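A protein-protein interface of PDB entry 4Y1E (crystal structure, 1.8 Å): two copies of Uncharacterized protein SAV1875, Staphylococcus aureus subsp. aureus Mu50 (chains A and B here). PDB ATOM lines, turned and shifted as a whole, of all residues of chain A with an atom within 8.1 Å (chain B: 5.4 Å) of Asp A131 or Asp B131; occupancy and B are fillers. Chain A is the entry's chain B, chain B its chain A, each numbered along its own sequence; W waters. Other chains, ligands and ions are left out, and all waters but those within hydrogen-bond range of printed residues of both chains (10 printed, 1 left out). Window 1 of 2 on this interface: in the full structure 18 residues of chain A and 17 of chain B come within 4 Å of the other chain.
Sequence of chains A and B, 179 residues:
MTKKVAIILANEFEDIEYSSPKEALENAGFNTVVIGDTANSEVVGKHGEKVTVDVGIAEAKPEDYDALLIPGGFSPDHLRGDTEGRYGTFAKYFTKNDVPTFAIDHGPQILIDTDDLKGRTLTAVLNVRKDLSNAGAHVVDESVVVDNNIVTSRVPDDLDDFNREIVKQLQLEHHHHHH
NH1 of Arg B80 is in salt-bridge range of OD2 of Asp A131 (2.8 Å). The side-chain amide oxygen of Asn B127 lies close to the backbone carbonyl oxygen of Asp A77 (2.7 Å). NH1 of Arg A80 lies within salt-bridge range of OD2 of Asp B131 (2.8 Å).
The guanidinium group (NE) of Arg B80 is in hydrogen-bond range of the backbone carbonyl oxygen (O) of Gln B109. NE of Arg A80 sits at hydrogen-bond distance from O of Gln A109 (3.3 Å). The guanidinium group (NH2) of Arg A80 is in salt-bridge range of the side-chain carboxylate (OD1) of Asp A113 (2.9 Å).
Among the printed residues, pairs that only touch across the chains: Ile A112 with Asp B131 (3.4 Å), Asp A131 with Ile B112 (3.5 Å), Ala A135 with Asn B134 (3.5 Å), Arg A80 with Asn B127 (3.6 Å), Asn A134 with Asn B134 (3.6 Å), Asn A134 with Ile B112 (3.6 Å), Asn A134 with Ala B135 (3.6 Å), Asn A127 with Arg B80 (3.6 Å), Ile A112 with Asn B134 (3.6 Å), Asp A131 with Asp B131 (3.8 Å), Asp A113 with Lys B130 (3.8 Å), Ile A112 with Lys B130 (3.9 Å), Lys A130 with Arg B80 (3.9 Å) and Lys A130 with Ile B112 (3.996 Å).
Of the printed residues of chain B, Asp A77 touches Asn B127 (2.7 Å). Pro A108 touches none of the printed residues of chain B. Of the printed residues of chain B, Ile A112 touches Lys B130 (3.9 Å), Asp B131 (3.4 Å) and Asn B134 (3.6 Å). Of the printed residues of chain B, Asp A113 touches Lys B130 (3.8 Å). Of the printed residues of chain B, Ala A135 touches Asn B134 (3.5 Å). Of the printed residues of chain A, Arg B80 touches Asn A127 (3.6 Å), Lys A130 (3.9 Å) and Asp A131 (2.8 Å). Ser B133 touches none of the printed residues of chain A.
Hydrophobic or aromatic side chains of chain A that line the printed part of chain B: Ile A112 and Ala A135. Along chain A the printed residues that touch a printed residue of chain B span positions 77 to 135. Along chain B the printed residues that touch a printed residue of chain A span positions 80 to 135.
Ile A112 touches Lys B130, and with the chains exchanged Lys A130 touches Ile B112. Ile A112 touches Asp B131, and with the chains exchanged Asp A131 touches Ile B112. Lys A130 touches Arg B80, but with the chains exchanged Arg A80 does not touch Lys B130 (4.2 Å). Asn A134 touches Ala B135, and with the chains exchanged Ala A135 touches Asn B134.
Water W4 lies within hydrogen-bond range of OD2 of Asp A131 (2.6 Å), NE2 of Gln A109 (2.8 Å) and OD2 of Asp B131 (3.0 Å). Water W3 lies within hydrogen-bond range of OD1 of Asp A77 (2.7 Å), NH1 of Arg A80 (2.9 Å) and O of Asn B127 (3.2 Å). Water W1 lies within hydrogen-bond range of ND2 of Asn A134, O of Asp B131 and OD1 of Asp A131. Water W2 bridges the backbone carbonyl oxygen of Ile B112 (2.8 Å) and the side-chain amide nitrogen of Asn A134 (3.1 Å). Water W5 lies within hydrogen-bond range of O of Ile A112 and ND2 of Asn B134. Water W6 lies within hydrogen-bond range of the backbone carbonyl oxygen of Asn A127 (2.9 Å) and the guanidinium group of Arg B80 (3.0 Å).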
ATOM      1  N   ASP A  77      21.973   4.516 -31.400  1.00  0.00           N
ATOM      2  CA  ASP A  77      22.470   5.242 -32.569  1.00  0.00           C
ATOM      3  C   ASP A  77      21.886   4.733 -33.872  1.00  0.00           C
ATOM      4  O   ASP A  77      21.491   5.525 -34.710  1.00  0.00           O
ATOM      5  CB  ASP A  77      24.002   5.271 -32.654  1.00  0.00           C
ATOM      6  CG  ASP A  77      24.493   6.221 -33.751  1.00  0.00           C
ATOM      7  OD1 ASP A  77      24.528   7.435 -33.520  1.00  0.00           O
ATOM      8  OD2 ASP A  77      24.735   5.754 -34.871  1.00  0.00           O
ATOM      9  N   ARG A  80      18.288   5.784 -34.310  1.00  0.00           N
ATOM     10  CA  ARG A  80      18.136   7.197 -34.658  1.00  0.00           C
ATOM     11  C   ARG A  80      18.471   7.409 -36.125  1.00  0.00           C
ATOM     12  O   ARG A  80      18.211   8.475 -36.677  1.00  0.00           O
ATOM     13  CB  ARG A  80      19.069   8.057 -33.782  1.00  0.00           C
ATOM     14  CG  ARG A  80      18.715   7.963 -32.295  1.00  0.00           C
ATOM     15  CD  ARG A  80      19.603   8.884 -31.466  1.00  0.00           C
ATOM     16  NE  ARG A  80      19.167  10.279 -31.584  1.00  0.00           N
ATOM     17  CZ  ARG A  80      19.923  11.326 -31.250  1.00  0.00           C
ATOM     18  NH1 ARG A  80      21.223  11.148 -30.972  1.00  0.00           N
ATOM     19  NH2 ARG A  80      19.369  12.528 -31.118  1.00  0.00           N
ATOM     20  N   PRO A 108      19.268   7.013 -23.497  1.00  0.00           N
ATOM     21  CA  PRO A 108      18.586   8.308 -23.513  1.00  0.00           C
ATOM     22  C   PRO A 108      18.724   9.107 -24.823  1.00  0.00           C
ATOM     23  O   PRO A 108      18.023  10.108 -24.999  1.00  0.00           O
ATOM     24  CB  PRO A 108      19.213   9.062 -22.331  1.00  0.00           C
ATOM     25  CG  PRO A 108      19.654   7.951 -21.396  1.00  0.00           C
ATOM     26  CD  PRO A 108      20.129   6.849 -22.318  1.00  0.00           C
ATOM     27  N   GLN A 109      19.679   8.754 -25.687  1.00  0.00           N
ATOM     28  CA  GLN A 109      19.787   9.436 -26.986  1.00  0.00           C
ATOM     29  C   GLN A 109      18.472   9.385 -27.792  1.00  0.00           C
ATOM     30  O   GLN A 109      18.085  10.372 -28.435  1.00  0.00           O
ATOM     31  CB  GLN A 109      20.915   8.829 -27.821  1.00  0.00           C
ATOM     32  CG  GLN A 109      22.308   9.130 -27.282  1.00  0.00           C
ATOM     33  CD  GLN A 109      23.363   8.623 -28.231  1.00  0.00           C
ATOM     34  OE1 GLN A 109      23.569   7.414 -28.351  1.00  0.00           O
ATOM     35  NE2 GLN A 109      24.030   9.545 -28.931  1.00  0.00           N
ATOM     36  N   ILE A 110      17.735   8.287 -27.675  1.00  0.00           N
ATOM     37  CA  ILE A 110      16.431   8.222 -28.348  1.00  0.00           C
ATOM     38  C   ILE A 110      15.430   9.195 -27.720  1.00  0.00           C
ATOM     39  O   ILE A 110      14.675   9.836 -28.438  1.00  0.00           O
ATOM     40  CB  ILE A 110      15.856   6.794 -28.449  1.00  0.00           C
ATOM     41  CG1 ILE A 110      16.140   6.235 -29.854  1.00  0.00           C
ATOM     42  CG2 ILE A 110      14.335   6.807 -28.388  1.00  0.00           C
ATOM     43  CD1 ILE A 110      17.259   5.243 -29.876  1.00  0.00           C
ATOM     44  N   LEU A 111      15.584   9.483 -26.435  1.00  0.00           N
ATOM     45  CA  LEU A 111      14.652  10.411 -25.799  1.00  0.00           C
ATOM     46  C   LEU A 111      14.855  11.836 -26.269  1.00  0.00           C
ATOM     47  O   LEU A 111      13.945  12.666 -26.185  1.00  0.00           O
ATOM     48  CB  LEU A 111      14.706  10.325 -24.265  1.00  0.00           C
ATOM     49  CG  LEU A 111      14.491   8.938 -23.645  1.00  0.00           C
ATOM     50  CD1 LEU A 111      14.593   9.040 -22.120  1.00  0.00           C
ATOM     51  CD2 LEU A 111      13.129   8.391 -24.052  1.00  0.00           C
ATOM     52  N   ILE A 112      16.063  12.131 -26.752  1.00  0.00           N
ATOM     53  CA  ILE A 112      16.324  13.441 -27.322  1.00  0.00           C
ATOM     54  C   ILE A 112      15.331  13.694 -28.459  1.00  0.00           C
ATOM     55  O   ILE A 112      14.844  14.820 -28.652  1.00  0.00           O
ATOM     56  CB  ILE A 112      17.784  13.531 -27.810  1.00  0.00           C
ATOM     57  CG1 ILE A 112      18.696  13.564 -26.579  1.00  0.00           C
ATOM     58  CG2 ILE A 112      17.988  14.811 -28.591  1.00  0.00           C
ATOM     59  CD1 ILE A 112      20.176  13.498 -26.921  1.00  0.00           C
ATOM     60  N   ASP A 113      15.020  12.636 -29.193  1.00  0.00           N
ATOM     61  CA  ASP A 113      14.266  12.782 -30.424  1.00  0.00           C
ATOM     62  C   ASP A 113      12.783  13.037 -30.145  1.00  0.00           C
ATOM     63  O   ASP A 113      12.042  13.435 -31.051  1.00  0.00           O
ATOM     64  CB  ASP A 113      14.443  11.534 -31.277  1.00  0.00           C
ATOM     65  CG  ASP A 113      15.838  11.426 -31.864  1.00  0.00           C
ATOM     66  OD1 ASP A 113      16.544  12.454 -31.941  1.00  0.00           O
ATOM     67  OD2 ASP A 113      16.256  10.296 -32.166  1.00  0.00           O
ATOM     68  N   LEU A 117      12.434  16.719 -23.449  1.00  0.00           N
ATOM     69  CA  LEU A 117      13.395  16.644 -22.324  1.00  0.00           C
ATOM     70  C   LEU A 117      13.557  17.958 -21.582  1.00  0.00           C
ATOM     71  O   LEU A 117      14.195  18.003 -20.530  1.00  0.00           O
ATOM     72  CB  LEU A 117      14.770  16.103 -22.773  1.00  0.00           C
ATOM     73  CG  LEU A 117      14.807  14.671 -23.313  1.00  0.00           C
ATOM     74  CD1 LEU A 117      16.239  14.211 -23.586  1.00  0.00           C
ATOM     75  CD2 LEU A 117      14.102  13.700 -22.386  1.00  0.00           C
ATOM     76  N   LEU A 122      17.785  13.762 -15.789  1.00  0.00           N
ATOM     77  CA  LEU A 122      18.247  12.423 -16.082  1.00  0.00           C
ATOM     78  C   LEU A 122      19.747  12.266 -16.043  1.00  0.00           C
ATOM     79  O   LEU A 122      20.488  13.248 -15.895  1.00  0.00           O
ATOM     80  CB  LEU A 122      17.684  11.919 -17.414  1.00  0.00           C
ATOM     81  CG  LEU A 122      17.710  12.826 -18.623  1.00  0.00           C
ATOM     82  CD1 LEU A 122      19.151  13.227 -18.910  1.00  0.00           C
ATOM     83  CD2 LEU A 122      17.123  12.065 -19.812  1.00  0.00           C
ATOM     84  N   VAL A 125      25.317   7.771 -20.004  1.00  0.00           N
ATOM     85  CA  VAL A 125      26.760   7.661 -20.190  1.00  0.00           C
ATOM     86  C   VAL A 125      27.389   9.021 -20.478  1.00  0.00           C
ATOM     87  O   VAL A 125      26.719   9.874 -21.047  1.00  0.00           O
ATOM     88  CB  VAL A 125      27.107   6.614 -21.266  1.00  0.00           C
ATOM     89  CG1 VAL A 125      26.794   7.134 -22.664  1.00  0.00           C
ATOM     90  CG2 VAL A 125      28.575   6.232 -21.140  1.00  0.00           C
ATOM     91  N   LEU A 126      28.604   9.267 -19.948  1.00  0.00           N
ATOM     92  CA  LEU A 126      29.255  10.569 -20.112  1.00  0.00           C
ATOM     93  C   LEU A 126      29.186  11.012 -21.571  1.00  0.00           C
ATOM     94  O   LEU A 126      28.934  12.184 -21.849  1.00  0.00           O
ATOM     95  CB  LEU A 126      30.719  10.492 -19.698  1.00  0.00           C
ATOM     96  CG  LEU A 126      31.496  11.752 -20.061  1.00  0.00           C
ATOM     97  CD1 LEU A 126      30.948  12.912 -19.241  1.00  0.00           C
ATOM     98  CD2 LEU A 126      32.945  11.486 -19.690  1.00  0.00           C
ATOM     99  N   ASN A 127      29.418  10.073 -22.492  1.00  0.00           N
ATOM    100  CA  ASN A 127      29.586  10.426 -23.895  1.00  0.00           C
ATOM    101  C   ASN A 127      28.417  11.244 -24.472  1.00  0.00           C
ATOM    102  O   ASN A 127      28.583  11.893 -25.508  1.00  0.00           O
ATOM    103  CB  ASN A 127      29.809   9.196 -24.781  1.00  0.00           C
ATOM    104  CG  ASN A 127      30.846   8.213 -24.227  1.00  0.00           C
ATOM    105  OD1 ASN A 127      31.584   7.577 -25.016  1.00  0.00           O
ATOM    106  ND2 ASN A 127      30.733   7.880 -22.947  1.00  0.00           N
ATOM    107  N   VAL A 128      27.206  11.067 -23.928  1.00  0.00           N
ATOM    108  CA  VAL A 128      26.037  11.738 -24.497  1.00  0.00           C
ATOM    109  C   VAL A 128      25.441  12.836 -23.608  1.00  0.00           C
ATOM    110  O   VAL A 128      24.447  13.450 -23.976  1.00  0.00           O
ATOM    111  CB  VAL A 128      24.943  10.729 -24.893  1.00  0.00           C
ATOM    112  CG1 VAL A 128      25.565   9.594 -25.693  1.00  0.00           C
ATOM    113  CG2 VAL A 128      24.254  10.187 -23.658  1.00  0.00           C
ATOM    114  N   ARG A 129      26.067  13.126 -22.468  1.00  0.00           N
ATOM    115  CA  ARG A 129      25.446  14.080 -21.534  1.00  0.00           C
ATOM    116  C   ARG A 129      25.298  15.454 -22.150  1.00  0.00           C
ATOM    117  O   ARG A 129      24.353  16.184 -21.852  1.00  0.00           O
ATOM    118  CB  ARG A 129      26.238  14.162 -20.215  1.00  0.00           C
ATOM    119  CG  ARG A 129      26.083  12.883 -19.421  1.00  0.00           C
ATOM    120  CD  ARG A 129      26.822  12.924 -18.086  1.00  0.00           C
ATOM    121  NE  ARG A 129      26.887  11.560 -17.572  1.00  0.00           N
ATOM    122  CZ  ARG A 129      27.827  11.117 -16.750  1.00  0.00           C
ATOM    123  NH1 ARG A 129      28.743  11.969 -16.249  1.00  0.00           N
ATOM    124  NH2 ARG A 129      27.865   9.828 -16.438  1.00  0.00           N
ATOM    125  N   LYS A 130      26.320  15.905 -22.866  1.00  0.00           N
ATOM    126  CA  LYS A 130      26.249  17.239 -23.448  1.00  0.00           C
ATOM    127  C   LYS A 130      25.032  17.369 -24.364  1.00  0.00           C
ATOM    128  O   LYS A 130      24.394  18.436 -24.423  1.00  0.00           O
ATOM    129  CB  LYS A 130      27.532  17.524 -24.256  1.00  0.00           C
ATOM    130  CG  LYS A 130      27.508  18.858 -24.983  1.00  0.00           C
ATOM    131  CD  LYS A 130      27.449  20.010 -24.006  1.00  0.00           C
ATOM    132  CE  LYS A 130      28.796  20.670 -23.826  1.00  0.00           C
ATOM    133  NZ  LYS A 130      28.579  22.135 -23.897  1.00  0.00           N
ATOM    134  N   ASP A 131      24.724  16.317 -25.113  1.00  0.00           N
ATOM    135  CA  ASP A 131      23.600  16.384 -26.043  1.00  0.00           C
ATOM    136  C   ASP A 131      22.270  16.432 -25.280  1.00  0.00           C
ATOM    137  O   ASP A 131      21.321  17.063 -25.735  1.00  0.00           O
ATOM    138  CB  ASP A 131      23.628  15.180 -26.981  1.00  0.00           C
ATOM    139  CG  ASP A 131      24.791  15.244 -27.959  1.00  0.00           C
ATOM    140  OD1 ASP A 131      25.362  16.350 -28.121  1.00  0.00           O
ATOM    141  OD2 ASP A 131      25.265  14.171 -28.374  1.00  0.00           O
ATOM    142  N   LEU A 132      22.209  15.758 -24.129  1.00  0.00           N
ATOM    143  CA  LEU A 132      20.998  15.804 -23.279  1.00  0.00           C
ATOM    144  C   LEU A 132      20.810  17.192 -22.673  1.00  0.00           C
ATOM    145  O   LEU A 132      19.695  17.710 -22.635  1.00  0.00           O
ATOM    146  CB  LEU A 132      21.069  14.749 -22.157  1.00  0.00           C
ATOM    147  CG  LEU A 132      21.002  13.302 -22.684  1.00  0.00           C
ATOM    148  CD1 LEU A 132      21.532  12.349 -21.618  1.00  0.00           C
ATOM    149  CD2 LEU A 132      19.583  12.882 -23.099  1.00  0.00           C
ATOM    150  N   SER A 133      21.921  17.821 -22.260  1.00  0.00           N
ATOM    151  CA  SER A 133      21.869  19.180 -21.745  1.00  0.00           C
ATOM    152  C   SER A 133      21.417  20.133 -22.835  1.00  0.00           C
ATOM    153  O   SER A 133      20.695  21.097 -22.557  1.00  0.00           O
ATOM    154  CB  SER A 133      23.248  19.605 -21.249  1.00  0.00           C
ATOM    155  OG  SER A 133      23.480  18.933 -20.061  1.00  0.00           O
ATOM    156  N   ASN A 134      21.928  19.950 -24.053  1.00  0.00           N
ATOM    157  CA  ASN A 134      21.527  20.830 -25.152  1.00  0.00           C
ATOM    158  C   ASN A 134      20.070  20.642 -25.516  1.00  0.00           C
ATOM    159  O   ASN A 134      19.459  21.544 -26.085  1.00  0.00           O
ATOM    160  CB  ASN A 134      22.383  20.618 -26.415  1.00  0.00           C
ATOM    161  CG  ASN A 134      23.711  21.340 -26.354  1.00  0.00           C
ATOM    162  OD1 ASN A 134      23.895  22.292 -25.595  1.00  0.00           O
ATOM    163  ND2 ASN A 134      24.627  20.927 -27.212  1.00  0.00           N
ATOM    164  N   ALA A 135      19.524  19.464 -25.214  1.00  0.00           N
ATOM    165  CA  ALA A 135      18.093  19.188 -25.413  1.00  0.00           C
ATOM    166  C   ALA A 135      17.230  19.738 -24.270  1.00  0.00           C
ATOM    167  O   ALA A 135      16.015  19.575 -24.276  1.00  0.00           O
ATOM    168  CB  ALA A 135      17.865  17.670 -25.562  1.00  0.00           C
ATOM    169  N   GLY A 136      17.857  20.387 -23.300  1.00  0.00           N
ATOM    170  CA  GLY A 136      17.118  21.082 -22.241  1.00  0.00           C
ATOM    171  C   GLY A 136      16.973  20.289 -20.946  1.00  0.00           C
ATOM    172  O   GLY A 136      16.439  20.796 -19.966  1.00  0.00           O
ATOM    173  N   ALA A 137      17.533  19.081 -20.894  1.00  0.00           N
ATOM    174  CA  ALA A 137      17.470  18.278 -19.656  1.00  0.00           C
ATOM    175  C   ALA A 137      18.434  18.810 -18.609  1.00  0.00           C
ATOM    176  O   ALA A 137      19.461  19.431 -18.952  1.00  0.00           O
ATOM    177  CB  ALA A 137      17.799  16.816 -19.949  1.00  0.00           C
ATOM    178  N   VAL A 139      21.055  17.483 -16.433  1.00  0.00           N
ATOM    179  CA  VAL A 139      21.807  16.220 -16.461  1.00  0.00           C
ATOM    180  C   VAL A 139      22.655  16.114 -15.208  1.00  0.00           C
ATOM    181  O   VAL A 139      23.261  17.102 -14.765  1.00  0.00           O
ATOM    182  CB  VAL A 139      22.738  16.151 -17.691  1.00  0.00           C
ATOM    183  CG1 VAL A 139      23.521  14.850 -17.696  1.00  0.00           C
ATOM    184  CG2 VAL A 139      21.928  16.299 -18.965  1.00  0.00           C
ATOM    185  N   ARG B  80      34.331  11.354 -27.179  1.00  0.00           N
ATOM    186  CA  ARG B  80      33.520  12.188 -26.292  1.00  0.00           C
ATOM    187  C   ARG B  80      33.338  11.495 -24.941  1.00  0.00           C
ATOM    188  O   ARG B  80      32.821  12.092 -23.982  1.00  0.00           O
ATOM    189  CB  ARG B  80      32.151  12.471 -26.948  1.00  0.00           C
ATOM    190  CG  ARG B  80      32.273  13.365 -28.182  1.00  0.00           C
ATOM    191  CD  ARG B  80      30.930  13.566 -28.893  1.00  0.00           C
ATOM    192  NE  ARG B  80      30.163  14.621 -28.216  1.00  0.00           N
ATOM    193  CZ  ARG B  80      28.845  14.811 -28.301  1.00  0.00           C
ATOM    194  NH1 ARG B  80      28.051  13.881 -28.834  1.00  0.00           N
ATOM    195  NH2 ARG B  80      28.310  15.889 -27.721  1.00  0.00           N
ATOM    196  N   GLN B 109      29.812  15.328 -34.279  1.00  0.00           N
ATOM    197  CA  GLN B 109      29.494  15.220 -32.857  1.00  0.00           C
ATOM    198  C   GLN B 109      30.561  15.915 -32.004  1.00  0.00           C
ATOM    199  O   GLN B 109      30.236  16.520 -30.981  1.00  0.00           O
ATOM    200  CB  GLN B 109      29.383  13.773 -32.405  1.00  0.00           C
ATOM    201  CG  GLN B 109      28.123  13.096 -32.888  1.00  0.00           C
ATOM    202  CD  GLN B 109      28.057  11.663 -32.409  1.00  0.00           C
ATOM    203  OE1 GLN B 109      28.898  10.832 -32.775  1.00  0.00           O
ATOM    204  NE2 GLN B 109      27.109  11.381 -31.512  1.00  0.00           N
ATOM    205  N   ILE B 112      30.103  19.643 -31.525  1.00  0.00           N
ATOM    206  CA  ILE B 112      29.143  20.054 -30.496  1.00  0.00           C
ATOM    207  C   ILE B 112      29.892  20.510 -29.241  1.00  0.00           C
ATOM    208  O   ILE B 112      29.505  21.504 -28.598  1.00  0.00           O
ATOM    209  CB  ILE B 112      28.162  18.901 -30.160  1.00  0.00           C
ATOM    210  CG1 ILE B 112      27.267  18.615 -31.372  1.00  0.00           C
ATOM    211  CG2 ILE B 112      27.301  19.273 -28.952  1.00  0.00           C
ATOM    212  CD1 ILE B 112      26.491  17.313 -31.279  1.00  0.00           C
ATOM    213  N   ASN B 127      21.585  10.394 -38.078  1.00  0.00           N
ATOM    214  CA  ASN B 127      21.555   9.976 -36.656  1.00  0.00           C
ATOM    215  C   ASN B 127      21.829  11.108 -35.660  1.00  0.00           C
ATOM    216  O   ASN B 127      21.485  10.989 -34.511  1.00  0.00           O
ATOM    217  CB  ASN B 127      22.554   8.858 -36.369  1.00  0.00           C
ATOM    218  CG  ASN B 127      22.468   7.700 -37.359  1.00  0.00           C
ATOM    219  OD1 ASN B 127      22.660   6.543 -36.967  1.00  0.00           O
ATOM    220  ND2 ASN B 127      22.276   8.002 -38.642  1.00  0.00           N
ATOM    221  N   VAL B 128      22.652  12.080 -36.039  1.00  0.00           N
ATOM    222  CA  VAL B 128      23.083  13.069 -35.085  1.00  0.00           C
ATOM    223  C   VAL B 128      22.573  14.476 -35.393  1.00  0.00           C
ATOM    224  O   VAL B 128      22.916  15.420 -34.693  1.00  0.00           O
ATOM    225  CB  VAL B 128      24.614  13.076 -34.886  1.00  0.00           C
ATOM    226  CG1 VAL B 128      25.104  11.687 -34.455  1.00  0.00           C
ATOM    227  CG2 VAL B 128      25.345  13.592 -36.122  1.00  0.00           C
ATOM    228  N   ARG B 129      21.814  14.637 -36.478  1.00  0.00           N
ATOM    229  CA  ARG B 129      21.413  15.976 -36.902  1.00  0.00           C
ATOM    230  C   ARG B 129      20.634  16.710 -35.792  1.00  0.00           C
ATOM    231  O   ARG B 129      20.752  17.927 -35.643  1.00  0.00           O
ATOM    232  CB  ARG B 129      20.580  15.910 -38.188  1.00  0.00           C
ATOM    233  CG  ARG B 129      21.448  15.758 -39.418  1.00  0.00           C
ATOM    234  CD  ARG B 129      20.614  15.777 -40.708  1.00  0.00           C
ATOM    235  NE  ARG B 129      21.394  15.060 -41.692  1.00  0.00           N
ATOM    236  CZ  ARG B 129      20.899  14.284 -42.638  1.00  0.00           C
ATOM    237  NH1 ARG B 129      19.586  14.291 -42.899  1.00  0.00           N
ATOM    238  NH2 ARG B 129      21.732  13.539 -43.353  1.00  0.00           N
ATOM    239  N   LYS B 130      19.777  15.988 -35.071  1.00  0.00           N
ATOM    240  CA  LYS B 130      18.985  16.641 -34.028  1.00  0.00           C
ATOM    241  C   LYS B 130      19.873  17.198 -32.911  1.00  0.00           C
ATOM    242  O   LYS B 130      19.611  18.286 -32.380  1.00  0.00           O
ATOM    243  CB  LYS B 130      17.938  15.683 -33.436  1.00  0.00           C
ATOM    244  CG  LYS B 130      17.267  16.203 -32.170  1.00  0.00           C
ATOM    245  CD  LYS B 130      16.653  17.593 -32.313  1.00  0.00           C
ATOM    246  CE  LYS B 130      15.429  17.603 -33.217  1.00  0.00           C
ATOM    247  NZ  LYS B 130      14.405  16.570 -32.898  1.00  0.00           N
ATOM    248  N   ASP B 131      20.986  16.521 -32.641  1.00  0.00           N
ATOM    249  CA  ASP B 131      21.884  16.991 -31.591  1.00  0.00           C
ATOM    250  C   ASP B 131      22.660  18.217 -32.079  1.00  0.00           C
ATOM    251  O   ASP B 131      22.934  19.137 -31.314  1.00  0.00           O
ATOM    252  CB  ASP B 131      22.863  15.876 -31.180  1.00  0.00           C
ATOM    253  CG  ASP B 131      22.150  14.612 -30.706  1.00  0.00           C
ATOM    254  OD1 ASP B 131      21.127  14.723 -29.990  1.00  0.00           O
ATOM    255  OD2 ASP B 131      22.649  13.502 -31.010  1.00  0.00           O
ATOM    256  N   LEU B 132      23.004  18.241 -33.361  1.00  0.00           N
ATOM    257  CA  LEU B 132      23.584  19.443 -33.951  1.00  0.00           C
ATOM    258  C   LEU B 132      22.614  20.622 -33.866  1.00  0.00           C
ATOM    259  O   LEU B 132      23.012  21.738 -33.560  1.00  0.00           O
ATOM    260  CB  LEU B 132      23.899  19.179 -35.427  1.00  0.00           C
ATOM    261  CG  LEU B 132      25.307  18.865 -35.897  1.00  0.00           C
ATOM    262  CD1 LEU B 132      26.424  18.889 -34.845  1.00  0.00           C
ATOM    263  CD2 LEU B 132      25.369  17.713 -36.883  1.00  0.00           C
ATOM    264  N   SER B 133      21.340  20.379 -34.176  1.00  0.00           N
ATOM    265  CA  SER B 133      20.357  21.451 -34.118  1.00  0.00           C
ATOM    266  C   SER B 133      20.147  21.918 -32.674  1.00  0.00           C
ATOM    267  O   SER B 133      20.067  23.125 -32.401  1.00  0.00           O
ATOM    268  CB  SER B 133      19.022  21.000 -34.736  1.00  0.00           C
ATOM    269  OG  SER B 133      18.180  22.135 -34.859  1.00  0.00           O
ATOM    270  N   ASN B 134      20.227  20.983 -31.724  1.00  0.00           N
ATOM    271  CA  ASN B 134      20.120  21.346 -30.313  1.00  0.00           C
ATOM    272  C   ASN B 134      21.341  22.132 -29.841  1.00  0.00           C
ATOM    273  O   ASN B 134      21.250  22.917 -28.896  1.00  0.00           O
ATOM    274  CB  ASN B 134      19.894  20.122 -29.418  1.00  0.00           C
ATOM    275  CG  ASN B 134      18.457  19.623 -29.475  1.00  0.00           C
ATOM    276  OD1 ASN B 134      17.550  20.377 -29.841  1.00  0.00           O
ATOM    277  ND2 ASN B 134      18.218  18.431 -28.960  1.00  0.00           N
ATOM    278  N   ALA B 135      22.438  22.022 -30.576  1.00  0.00           N
ATOM    279  CA  ALA B 135      23.655  22.756 -30.215  1.00  0.00           C
ATOM    280  C   ALA B 135      23.635  24.132 -30.867  1.00  0.00           C
ATOM    281  O   ALA B 135      24.603  24.892 -30.743  1.00  0.00           O
ATOM    282  CB  ALA B 135      24.905  22.004 -30.657  1.00  0.00           C
ATOM    283  N   GLY B 136      22.600  24.393 -31.658  1.00  0.00           N
ATOM    284  CA  GLY B 136      22.374  25.728 -32.201  1.00  0.00           C
ATOM    285  C   GLY B 136      22.809  25.913 -33.649  1.00  0.00           C
ATOM    286  O   GLY B 136      22.636  27.006 -34.212  1.00  0.00           O
HETATM  287  O   HOH W   1      23.809  18.721 -28.629  1.00  0.00           O
HETATM  288  O   HOH W   2      27.108  22.613 -27.802  1.00  0.00           O
HETATM  289  O   HOH W   3      22.833   9.120 -32.337  1.00  0.00           O
HETATM  290  O   HOH W   4      23.450  12.272 -28.368  1.00  0.00           O
HETATM  291  O   HOH W   5      15.379  17.553 -28.419  1.00  0.00           O
HETATM  292  O   HOH W   6      28.682  11.021 -28.297  1.00  0.00           O
HETATM  293  O   HOH W   7      26.510   8.574 -30.662  1.00  0.00           O
HETATM  294  O   HOH W   8      20.667  17.122 -28.400  1.00  0.00           O
HETATM  295  O   HOH W   9      25.347  13.590 -31.028  1.00  0.00           O
HETATM  296  O   HOH W  10      15.066  13.955 -33.861  1.00  0.00           O
